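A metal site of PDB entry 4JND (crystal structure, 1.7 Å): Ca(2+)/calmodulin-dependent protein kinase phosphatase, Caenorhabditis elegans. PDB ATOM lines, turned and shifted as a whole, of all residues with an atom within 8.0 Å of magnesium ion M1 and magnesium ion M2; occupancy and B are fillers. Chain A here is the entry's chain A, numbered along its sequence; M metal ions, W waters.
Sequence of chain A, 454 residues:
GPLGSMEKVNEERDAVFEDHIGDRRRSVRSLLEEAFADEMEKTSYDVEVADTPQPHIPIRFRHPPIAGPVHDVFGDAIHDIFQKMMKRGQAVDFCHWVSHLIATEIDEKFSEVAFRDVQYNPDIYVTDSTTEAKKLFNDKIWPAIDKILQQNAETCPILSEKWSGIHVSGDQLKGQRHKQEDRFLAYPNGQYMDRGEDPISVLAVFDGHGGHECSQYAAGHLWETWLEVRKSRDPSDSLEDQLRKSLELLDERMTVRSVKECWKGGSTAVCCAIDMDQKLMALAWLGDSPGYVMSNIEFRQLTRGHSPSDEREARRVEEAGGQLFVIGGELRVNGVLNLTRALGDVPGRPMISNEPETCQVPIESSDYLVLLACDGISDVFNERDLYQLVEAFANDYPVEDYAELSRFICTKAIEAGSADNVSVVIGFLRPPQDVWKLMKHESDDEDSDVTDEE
The side-chain hydroxyl (OG) of Ser 267 sits close to the backbone carbonyl oxygen (O) of Asp 207, at 3.4 Å.
The backbone NH (N) of Gly 208 is in hydrogen-bond range of the backbone carbonyl oxygen (O) of Glu 181, at 2.9 Å.
The guanidinium group of Arg 177 is in salt-bridge range of the side-chain carboxylate of Asp 420 (3.1 Å).
OG1 of Thr 268 sits at hydrogen-bond distance from N of Asp 207 (2.9 Å).
Two residues have an atom within 4 Å of magnesium ion M2: Asp 207 and Gly 208.
Magnesium ion M1 is bound by the side-chain carboxylate (OD2) of Asp 207 (2.1 Å).
OD2 of Asp 420 binds magnesium ion M1, at 2.2 Å.
Water W4 binds magnesium ion M1 (2.2 Å).
Water W6 binds magnesium ion M1 (2.2 Å).
OD1 of Asp 375 is bound to magnesium ion M1 (2.2 Å).
Water W1 is bound to magnesium ion M1 (2.2 Å).
Water W2 is bound to magnesium ion M2 (2.1 Å).
Magnesium ion M2 is bound by OD1 of Asp 207, at 2.1 Å.
Water W5 binds magnesium ion M2, at 2.1 Å.
O of Gly 208 binds magnesium ion M2 (2.1 Å).
Water W1 binds magnesium ion M2 (2.2 Å).
Water W3 is bound to magnesium ion M2 (2.2 Å).
Magnesium ion M2 has six donor atoms within binding distance.
Water W2 bridges the side-chain amide nitrogen of Asn 421 and the side-chain carboxylate of Asp 182.
Water W3 bridges OE1 of Glu 181 and NH1 of Arg 177.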
ATOM      1  N   ARG A 177       7.046 -22.263 -39.746  1.00  0.00           N
ATOM      2  CA  ARG A 177       7.842 -23.441 -39.417  1.00  0.00           C
ATOM      3  C   ARG A 177       7.362 -24.621 -40.250  1.00  0.00           C
ATOM      4  O   ARG A 177       6.291 -24.590 -40.835  1.00  0.00           O
ATOM      5  CB  ARG A 177       7.700 -23.787 -37.934  1.00  0.00           C
ATOM      6  CG  ARG A 177       8.322 -22.785 -36.944  1.00  0.00           C
ATOM      7  CD  ARG A 177       9.835 -22.772 -37.112  1.00  0.00           C
ATOM      8  NE  ARG A 177      10.507 -21.837 -36.227  1.00  0.00           N
ATOM      9  CZ  ARG A 177      11.103 -22.163 -35.079  1.00  0.00           C
ATOM     10  NH1 ARG A 177      11.110 -23.434 -34.679  1.00  0.00           N
ATOM     11  NH2 ARG A 177      11.718 -21.244 -34.358  1.00  0.00           N
ATOM     12  N   LYS A 179       7.127 -27.871 -39.066  1.00  0.00           N
ATOM     13  CA  LYS A 179       6.346 -28.782 -38.251  1.00  0.00           C
ATOM     14  C   LYS A 179       5.918 -28.072 -36.973  1.00  0.00           C
ATOM     15  O   LYS A 179       6.579 -27.155 -36.511  1.00  0.00           O
ATOM     16  CB  LYS A 179       7.182 -30.017 -37.901  1.00  0.00           C
ATOM     17  CG  LYS A 179       6.345 -31.195 -37.461  1.00  0.00           C
ATOM     18  CD  LYS A 179       7.114 -32.083 -36.500  1.00  0.00           C
ATOM     19  CE  LYS A 179       8.530 -32.346 -36.982  1.00  0.00           C
ATOM     20  NZ  LYS A 179       9.336 -33.061 -35.951  1.00  0.00           N
ATOM     21  N   GLN A 180       4.797 -28.516 -36.416  1.00  0.00           N
ATOM     22  CA  GLN A 180       4.375 -28.037 -35.115  1.00  0.00           C
ATOM     23  C   GLN A 180       5.070 -28.871 -34.035  1.00  0.00           C
ATOM     24  O   GLN A 180       4.754 -30.046 -33.852  1.00  0.00           O
ATOM     25  CB  GLN A 180       2.846 -28.156 -34.988  1.00  0.00           C
ATOM     26  CG  GLN A 180       2.318 -27.769 -33.607  1.00  0.00           C
ATOM     27  CD  GLN A 180       2.714 -26.366 -33.221  1.00  0.00           C
ATOM     28  OE1 GLN A 180       3.772 -26.131 -32.629  1.00  0.00           O
ATOM     29  NE2 GLN A 180       1.863 -25.402 -33.568  1.00  0.00           N
ATOM     30  N   GLU A 181       6.049 -28.279 -33.366  1.00  0.00           N
ATOM     31  CA  GLU A 181       6.807 -28.992 -32.347  1.00  0.00           C
ATOM     32  C   GLU A 181       6.394 -28.599 -30.917  1.00  0.00           C
ATOM     33  O   GLU A 181       6.930 -29.151 -29.955  1.00  0.00           O
ATOM     34  CB  GLU A 181       8.316 -28.789 -32.551  1.00  0.00           C
ATOM     35  CG  GLU A 181       8.801 -29.306 -33.906  1.00  0.00           C
ATOM     36  CD  GLU A 181      10.281 -29.081 -34.116  1.00  0.00           C
ATOM     37  OE1 GLU A 181      10.701 -27.901 -34.069  1.00  0.00           O
ATOM     38  OE2 GLU A 181      11.015 -30.063 -34.306  1.00  0.00           O
ATOM     39  N   ASP A 182       5.454 -27.657 -30.780  1.00  0.00           N
ATOM     40  CA  ASP A 182       4.887 -27.263 -29.475  1.00  0.00           C
ATOM     41  C   ASP A 182       3.718 -28.207 -29.152  1.00  0.00           C
ATOM     42  O   ASP A 182       2.990 -28.652 -30.065  1.00  0.00           O
ATOM     43  CB  ASP A 182       4.238 -25.868 -29.529  1.00  0.00           C
ATOM     44  CG  ASP A 182       5.229 -24.697 -29.462  1.00  0.00           C
ATOM     45  OD1 ASP A 182       6.457 -24.874 -29.378  1.00  0.00           O
ATOM     46  OD2 ASP A 182       4.713 -23.552 -29.481  1.00  0.00           O
ATOM     47  N   PHE A 206       4.581 -27.172 -23.812  1.00  0.00           N
ATOM     48  CA  PHE A 206       5.849 -27.873 -24.054  1.00  0.00           C
ATOM     49  C   PHE A 206       6.354 -27.433 -25.413  1.00  0.00           C
ATOM     50  O   PHE A 206       5.731 -27.704 -26.428  1.00  0.00           O
ATOM     51  CB  PHE A 206       5.624 -29.397 -24.062  1.00  0.00           C
ATOM     52  CG  PHE A 206       4.969 -29.924 -22.802  1.00  0.00           C
ATOM     53  CD1 PHE A 206       5.689 -30.056 -21.631  1.00  0.00           C
ATOM     54  CD2 PHE A 206       3.635 -30.330 -22.812  1.00  0.00           C
ATOM     55  CE1 PHE A 206       5.091 -30.537 -20.459  1.00  0.00           C
ATOM     56  CE2 PHE A 206       3.026 -30.830 -21.650  1.00  0.00           C
ATOM     57  CZ  PHE A 206       3.748 -30.930 -20.486  1.00  0.00           C
ATOM     58  N   ASP A 207       7.514 -26.776 -25.430  1.00  0.00           N
ATOM     59  CA  ASP A 207       8.114 -26.331 -26.676  1.00  0.00           C
ATOM     60  C   ASP A 207       9.236 -27.282 -27.116  1.00  0.00           C
ATOM     61  O   ASP A 207      10.341 -27.228 -26.575  1.00  0.00           O
ATOM     62  CB  ASP A 207       8.643 -24.915 -26.509  1.00  0.00           C
ATOM     63  CG  ASP A 207       9.303 -24.391 -27.757  1.00  0.00           C
ATOM     64  OD1 ASP A 207       9.526 -25.184 -28.663  1.00  0.00           O
ATOM     65  OD2 ASP A 207       9.572 -23.186 -27.815  1.00  0.00           O
ATOM     66  N   GLY A 208       8.943 -28.145 -28.082  1.00  0.00           N
ATOM     67  CA  GLY A 208       9.902 -29.129 -28.543  1.00  0.00           C
ATOM     68  C   GLY A 208      11.001 -28.507 -29.396  1.00  0.00           C
ATOM     69  O   GLY A 208      10.770 -27.515 -30.073  1.00  0.00           O
ATOM     70  N   HIS A 209      12.190 -29.089 -29.354  1.00  0.00           N
ATOM     71  CA  HIS A 209      13.252 -28.745 -30.299  1.00  0.00           C
ATOM     72  C   HIS A 209      13.888 -30.030 -30.787  1.00  0.00           C
ATOM     73  O   HIS A 209      13.912 -31.021 -30.055  1.00  0.00           O
ATOM     74  CB  HIS A 209      14.321 -27.850 -29.648  1.00  0.00           C
ATOM     75  CG  HIS A 209      14.856 -28.384 -28.354  1.00  0.00           C
ATOM     76  ND1 HIS A 209      14.451 -27.910 -27.126  1.00  0.00           N
ATOM     77  CD2 HIS A 209      15.771 -29.358 -28.101  1.00  0.00           C
ATOM     78  CE1 HIS A 209      15.089 -28.570 -26.176  1.00  0.00           C
ATOM     79  NE2 HIS A 209      15.885 -29.449 -26.736  1.00  0.00           N
ATOM     80  N   GLY A 210      14.376 -30.040 -32.029  1.00  0.00           N
ATOM     81  CA  GLY A 210      14.984 -31.238 -32.583  1.00  0.00           C
ATOM     82  C   GLY A 210      13.997 -32.374 -32.801  1.00  0.00           C
ATOM     83  O   GLY A 210      14.367 -33.549 -32.810  1.00  0.00           O
ATOM     84  N   GLY A 211      12.728 -32.007 -32.994  1.00  0.00           N
ATOM     85  CA  GLY A 211      11.675 -32.973 -33.219  1.00  0.00           C
ATOM     86  C   GLY A 211      10.510 -32.696 -32.281  1.00  0.00           C
ATOM     87  O   GLY A 211      10.586 -31.851 -31.389  1.00  0.00           O
ATOM     88  N   SER A 215       7.951 -33.331 -26.818  1.00  0.00           N
ATOM     89  CA  SER A 215       6.795 -32.535 -26.458  1.00  0.00           C
ATOM     90  C   SER A 215       5.504 -33.367 -26.592  1.00  0.00           C
ATOM     91  O   SER A 215       4.603 -33.264 -25.753  1.00  0.00           O
ATOM     92  CB  SER A 215       6.755 -31.236 -27.290  1.00  0.00           C
ATOM     93  OG  SER A 215       6.737 -31.509 -28.687  1.00  0.00           O
ATOM     94  N   GLY A 266      14.514 -32.537 -27.551  1.00  0.00           N
ATOM     95  CA  GLY A 266      14.047 -32.348 -26.191  1.00  0.00           C
ATOM     96  C   GLY A 266      12.883 -31.389 -26.217  1.00  0.00           C
ATOM     97  O   GLY A 266      12.339 -31.078 -27.288  1.00  0.00           O
ATOM     98  N   SER A 267      12.474 -30.941 -25.043  1.00  0.00           N
ATOM     99  CA  SER A 267      11.358 -30.002 -24.976  1.00  0.00           C
ATOM    100  C   SER A 267      11.510 -29.118 -23.737  1.00  0.00           C
ATOM    101  O   SER A 267      12.037 -29.549 -22.711  1.00  0.00           O
ATOM    102  CB  SER A 267      10.050 -30.759 -24.912  1.00  0.00           C
ATOM    103  OG  SER A 267       8.944 -29.876 -24.874  1.00  0.00           O
ATOM    104  N   THR A 268      11.030 -27.888 -23.824  1.00  0.00           N
ATOM    105  CA  THR A 268      10.834 -27.132 -22.598  1.00  0.00           C
ATOM    106  C   THR A 268       9.563 -27.659 -21.931  1.00  0.00           C
ATOM    107  O   THR A 268       8.791 -28.453 -22.516  1.00  0.00           O
ATOM    108  CB  THR A 268      10.548 -25.648 -22.856  1.00  0.00           C
ATOM    109  OG1 THR A 268       9.262 -25.541 -23.487  1.00  0.00           O
ATOM    110  CG2 THR A 268      11.602 -25.038 -23.750  1.00  0.00           C
ATOM    111  N   ASP A 288      12.619 -22.038 -21.460  1.00  0.00           N
ATOM    112  CA  ASP A 288      12.293 -20.634 -21.663  1.00  0.00           C
ATOM    113  C   ASP A 288      10.866 -20.369 -22.099  1.00  0.00           C
ATOM    114  O   ASP A 288      10.593 -19.331 -22.721  1.00  0.00           O
ATOM    115  CB  ASP A 288      13.241 -20.009 -22.690  1.00  0.00           C
ATOM    116  CG  ASP A 288      13.135 -20.670 -24.080  1.00  0.00           C
ATOM    117  OD1 ASP A 288      12.291 -21.568 -24.293  1.00  0.00           O
ATOM    118  OD2 ASP A 288      13.926 -20.296 -24.982  1.00  0.00           O
ATOM    119  N   SER A 289       9.962 -21.294 -21.810  1.00  0.00           N
ATOM    120  CA  SER A 289       8.542 -21.039 -22.053  1.00  0.00           C
ATOM    121  C   SER A 289       8.019 -20.367 -20.787  1.00  0.00           C
ATOM    122  O   SER A 289       8.089 -20.970 -19.710  1.00  0.00           O
ATOM    123  CB  SER A 289       7.799 -22.354 -22.315  1.00  0.00           C
ATOM    124  OG  SER A 289       8.305 -23.057 -23.465  1.00  0.00           O
ATOM    125  N   LEU A 339      19.207 -23.090 -24.490  1.00  0.00           N
ATOM    126  CA  LEU A 339      18.535 -23.403 -23.229  1.00  0.00           C
ATOM    127  C   LEU A 339      19.513 -24.112 -22.317  1.00  0.00           C
ATOM    128  O   LEU A 339      20.441 -24.751 -22.812  1.00  0.00           O
ATOM    129  CB  LEU A 339      17.369 -24.370 -23.471  1.00  0.00           C
ATOM    130  CG  LEU A 339      16.201 -23.980 -24.352  1.00  0.00           C
ATOM    131  CD1 LEU A 339      15.246 -25.159 -24.413  1.00  0.00           C
ATOM    132  CD2 LEU A 339      15.527 -22.753 -23.786  1.00  0.00           C
ATOM    133  N   CYS A 374       4.667 -20.391 -25.082  1.00  0.00           N
ATOM    134  CA  CYS A 374       6.029 -20.687 -25.519  1.00  0.00           C
ATOM    135  C   CYS A 374       6.742 -19.369 -25.816  1.00  0.00           C
ATOM    136  O   CYS A 374       6.125 -18.304 -25.856  1.00  0.00           O
ATOM    137  CB  CYS A 374       6.002 -21.554 -26.765  1.00  0.00           C
ATOM    138  SG  CYS A 374       5.321 -20.668 -28.138  1.00  0.00           S
ATOM    139  N   ASP A 375       8.049 -19.423 -26.046  1.00  0.00           N
ATOM    140  CA  ASP A 375       8.803 -18.233 -26.351  1.00  0.00           C
ATOM    141  C   ASP A 375       8.397 -17.545 -27.660  1.00  0.00           C
ATOM    142  O   ASP A 375       8.739 -16.384 -27.866  1.00  0.00           O
ATOM    143  CB  ASP A 375      10.296 -18.572 -26.363  1.00  0.00           C
ATOM    144  CG  ASP A 375      10.685 -19.495 -27.498  1.00  0.00           C
ATOM    145  OD1 ASP A 375       9.798 -20.187 -28.052  1.00  0.00           O
ATOM    146  OD2 ASP A 375      11.888 -19.502 -27.844  1.00  0.00           O
ATOM    147  N   GLY A 376       7.717 -18.264 -28.548  1.00  0.00           N
ATOM    148  CA  GLY A 376       7.180 -17.668 -29.759  1.00  0.00           C
ATOM    149  C   GLY A 376       6.275 -16.464 -29.485  1.00  0.00           C
ATOM    150  O   GLY A 376       6.173 -15.548 -30.319  1.00  0.00           O
ATOM    151  N   ILE A 377       5.613 -16.469 -28.341  1.00  0.00           N
ATOM    152  CA  ILE A 377       4.765 -15.361 -27.898  1.00  0.00           C
ATOM    153  C   ILE A 377       5.616 -14.250 -27.265  1.00  0.00           C
ATOM    154  O   ILE A 377       5.493 -13.081 -27.648  1.00  0.00           O
ATOM    155  CB  ILE A 377       3.703 -15.843 -26.875  1.00  0.00           C
ATOM    156  CG1 ILE A 377       2.818 -16.915 -27.521  1.00  0.00           C
ATOM    157  CG2 ILE A 377       2.852 -14.692 -26.361  1.00  0.00           C
ATOM    158  CD1 ILE A 377       1.947 -16.383 -28.643  1.00  0.00           C
ATOM    159  N   ASP A 379       8.675 -13.606 -27.619  1.00  0.00           N
ATOM    160  CA  ASP A 379       9.599 -13.017 -28.583  1.00  0.00           C
ATOM    161  C   ASP A 379       9.048 -11.685 -29.111  1.00  0.00           C
ATOM    162  O   ASP A 379       9.811 -10.806 -29.515  1.00  0.00           O
ATOM    163  CB  ASP A 379       9.848 -13.951 -29.782  1.00  0.00           C
ATOM    164  CG  ASP A 379      10.836 -15.063 -29.458  1.00  0.00           C
ATOM    165  OD1 ASP A 379      11.509 -15.002 -28.408  1.00  0.00           O
ATOM    166  OD2 ASP A 379      10.943 -16.009 -30.283  1.00  0.00           O
ATOM    167  N   SER A 418       6.316 -12.940 -35.216  1.00  0.00           N
ATOM    168  CA  SER A 418       6.948 -14.119 -34.597  1.00  0.00           C
ATOM    169  C   SER A 418       7.268 -15.146 -35.678  1.00  0.00           C
ATOM    170  O   SER A 418       6.445 -15.386 -36.576  1.00  0.00           O
ATOM    171  CB  SER A 418       6.055 -14.745 -33.536  1.00  0.00           C
ATOM    172  OG  SER A 418       6.709 -15.896 -33.021  1.00  0.00           O
ATOM    173  N   ALA A 419       8.446 -15.759 -35.593  1.00  0.00           N
ATOM    174  CA  ALA A 419       8.903 -16.695 -36.609  1.00  0.00           C
ATOM    175  C   ALA A 419       8.957 -18.128 -36.071  1.00  0.00           C
ATOM    176  O   ALA A 419       9.618 -19.003 -36.644  1.00  0.00           O
ATOM    177  CB  ALA A 419      10.272 -16.294 -37.125  1.00  0.00           C
ATOM    178  N   ASP A 420       8.244 -18.373 -34.979  1.00  0.00           N
ATOM    179  CA  ASP A 420       8.290 -19.664 -34.306  1.00  0.00           C
ATOM    180  C   ASP A 420       6.886 -20.274 -34.253  1.00  0.00           C
ATOM    181  O   ASP A 420       5.904 -19.610 -34.548  1.00  0.00           O
ATOM    182  CB  ASP A 420       8.756 -19.413 -32.873  1.00  0.00           C
ATOM    183  CG  ASP A 420       9.260 -20.666 -32.167  1.00  0.00           C
ATOM    184  OD1 ASP A 420       9.135 -21.806 -32.690  1.00  0.00           O
ATOM    185  OD2 ASP A 420       9.785 -20.472 -31.046  1.00  0.00           O
ATOM    186  N   ASN A 421       6.816 -21.558 -33.896  1.00  0.00           N
ATOM    187  CA  ASN A 421       5.567 -22.106 -33.388  1.00  0.00           C
ATOM    188  C   ASN A 421       5.067 -21.216 -32.217  1.00  0.00           C
ATOM    189  O   ASN A 421       5.854 -20.718 -31.409  1.00  0.00           O
ATOM    190  CB  ASN A 421       5.790 -23.528 -32.854  1.00  0.00           C
ATOM    191  CG  ASN A 421       6.236 -24.533 -33.934  1.00  0.00           C
ATOM    192  OD1 ASN A 421       5.839 -24.494 -35.125  1.00  0.00           O
ATOM    193  ND2 ASN A 421       7.043 -25.479 -33.491  1.00  0.00           N
ATOM    194  N   VAL A 422       3.751 -21.044 -32.099  1.00  0.00           N
ATOM    195  CA  VAL A 422       3.206 -20.256 -31.011  1.00  0.00           C
ATOM    196  C   VAL A 422       2.096 -21.045 -30.332  1.00  0.00           C
ATOM    197  O   VAL A 422       1.231 -21.622 -31.004  1.00  0.00           O
ATOM    198  CB  VAL A 422       2.657 -18.887 -31.489  1.00  0.00           C
ATOM    199  CG1 VAL A 422       3.812 -17.931 -31.874  1.00  0.00           C
ATOM    200  CG2 VAL A 422       1.687 -19.081 -32.646  1.00  0.00           C
ATOM    201  N   SER A 423       2.113 -21.066 -28.992  1.00  0.00           N
ATOM    202  CA  SER A 423       1.083 -21.775 -28.227  1.00  0.00           C
ATOM    203  C   SER A 423       0.766 -21.000 -26.967  1.00  0.00           C
ATOM    204  O   SER A 423       1.664 -20.425 -26.350  1.00  0.00           O
ATOM    205  CB  SER A 423       1.567 -23.167 -27.824  1.00  0.00           C
ATOM    206  OG  SER A 423       2.003 -23.906 -28.947  1.00  0.00           O
HETATM  207 MG    MG M   1       9.886 -21.899 -29.427  1.00  0.00          MG
HETATM  208 MG    MG M   2      10.445 -25.445 -30.536  1.00  0.00          MG
HETATM  209  O   HOH W   1      10.481 -23.343 -31.029  1.00  0.00           O
HETATM  210  O   HOH W   2       8.459 -25.601 -31.176  1.00  0.00           O
HETATM  211  O   HOH W   3      11.252 -25.829 -32.511  1.00  0.00           O
HETATM  212  O   HOH W   4      12.010 -21.825 -29.013  1.00  0.00           O
HETATM  213  O   HOH W   5      12.375 -25.019 -29.798  1.00  0.00           O
HETATM  214  O   HOH W   6       7.760 -22.224 -29.853  1.00  0.00           O
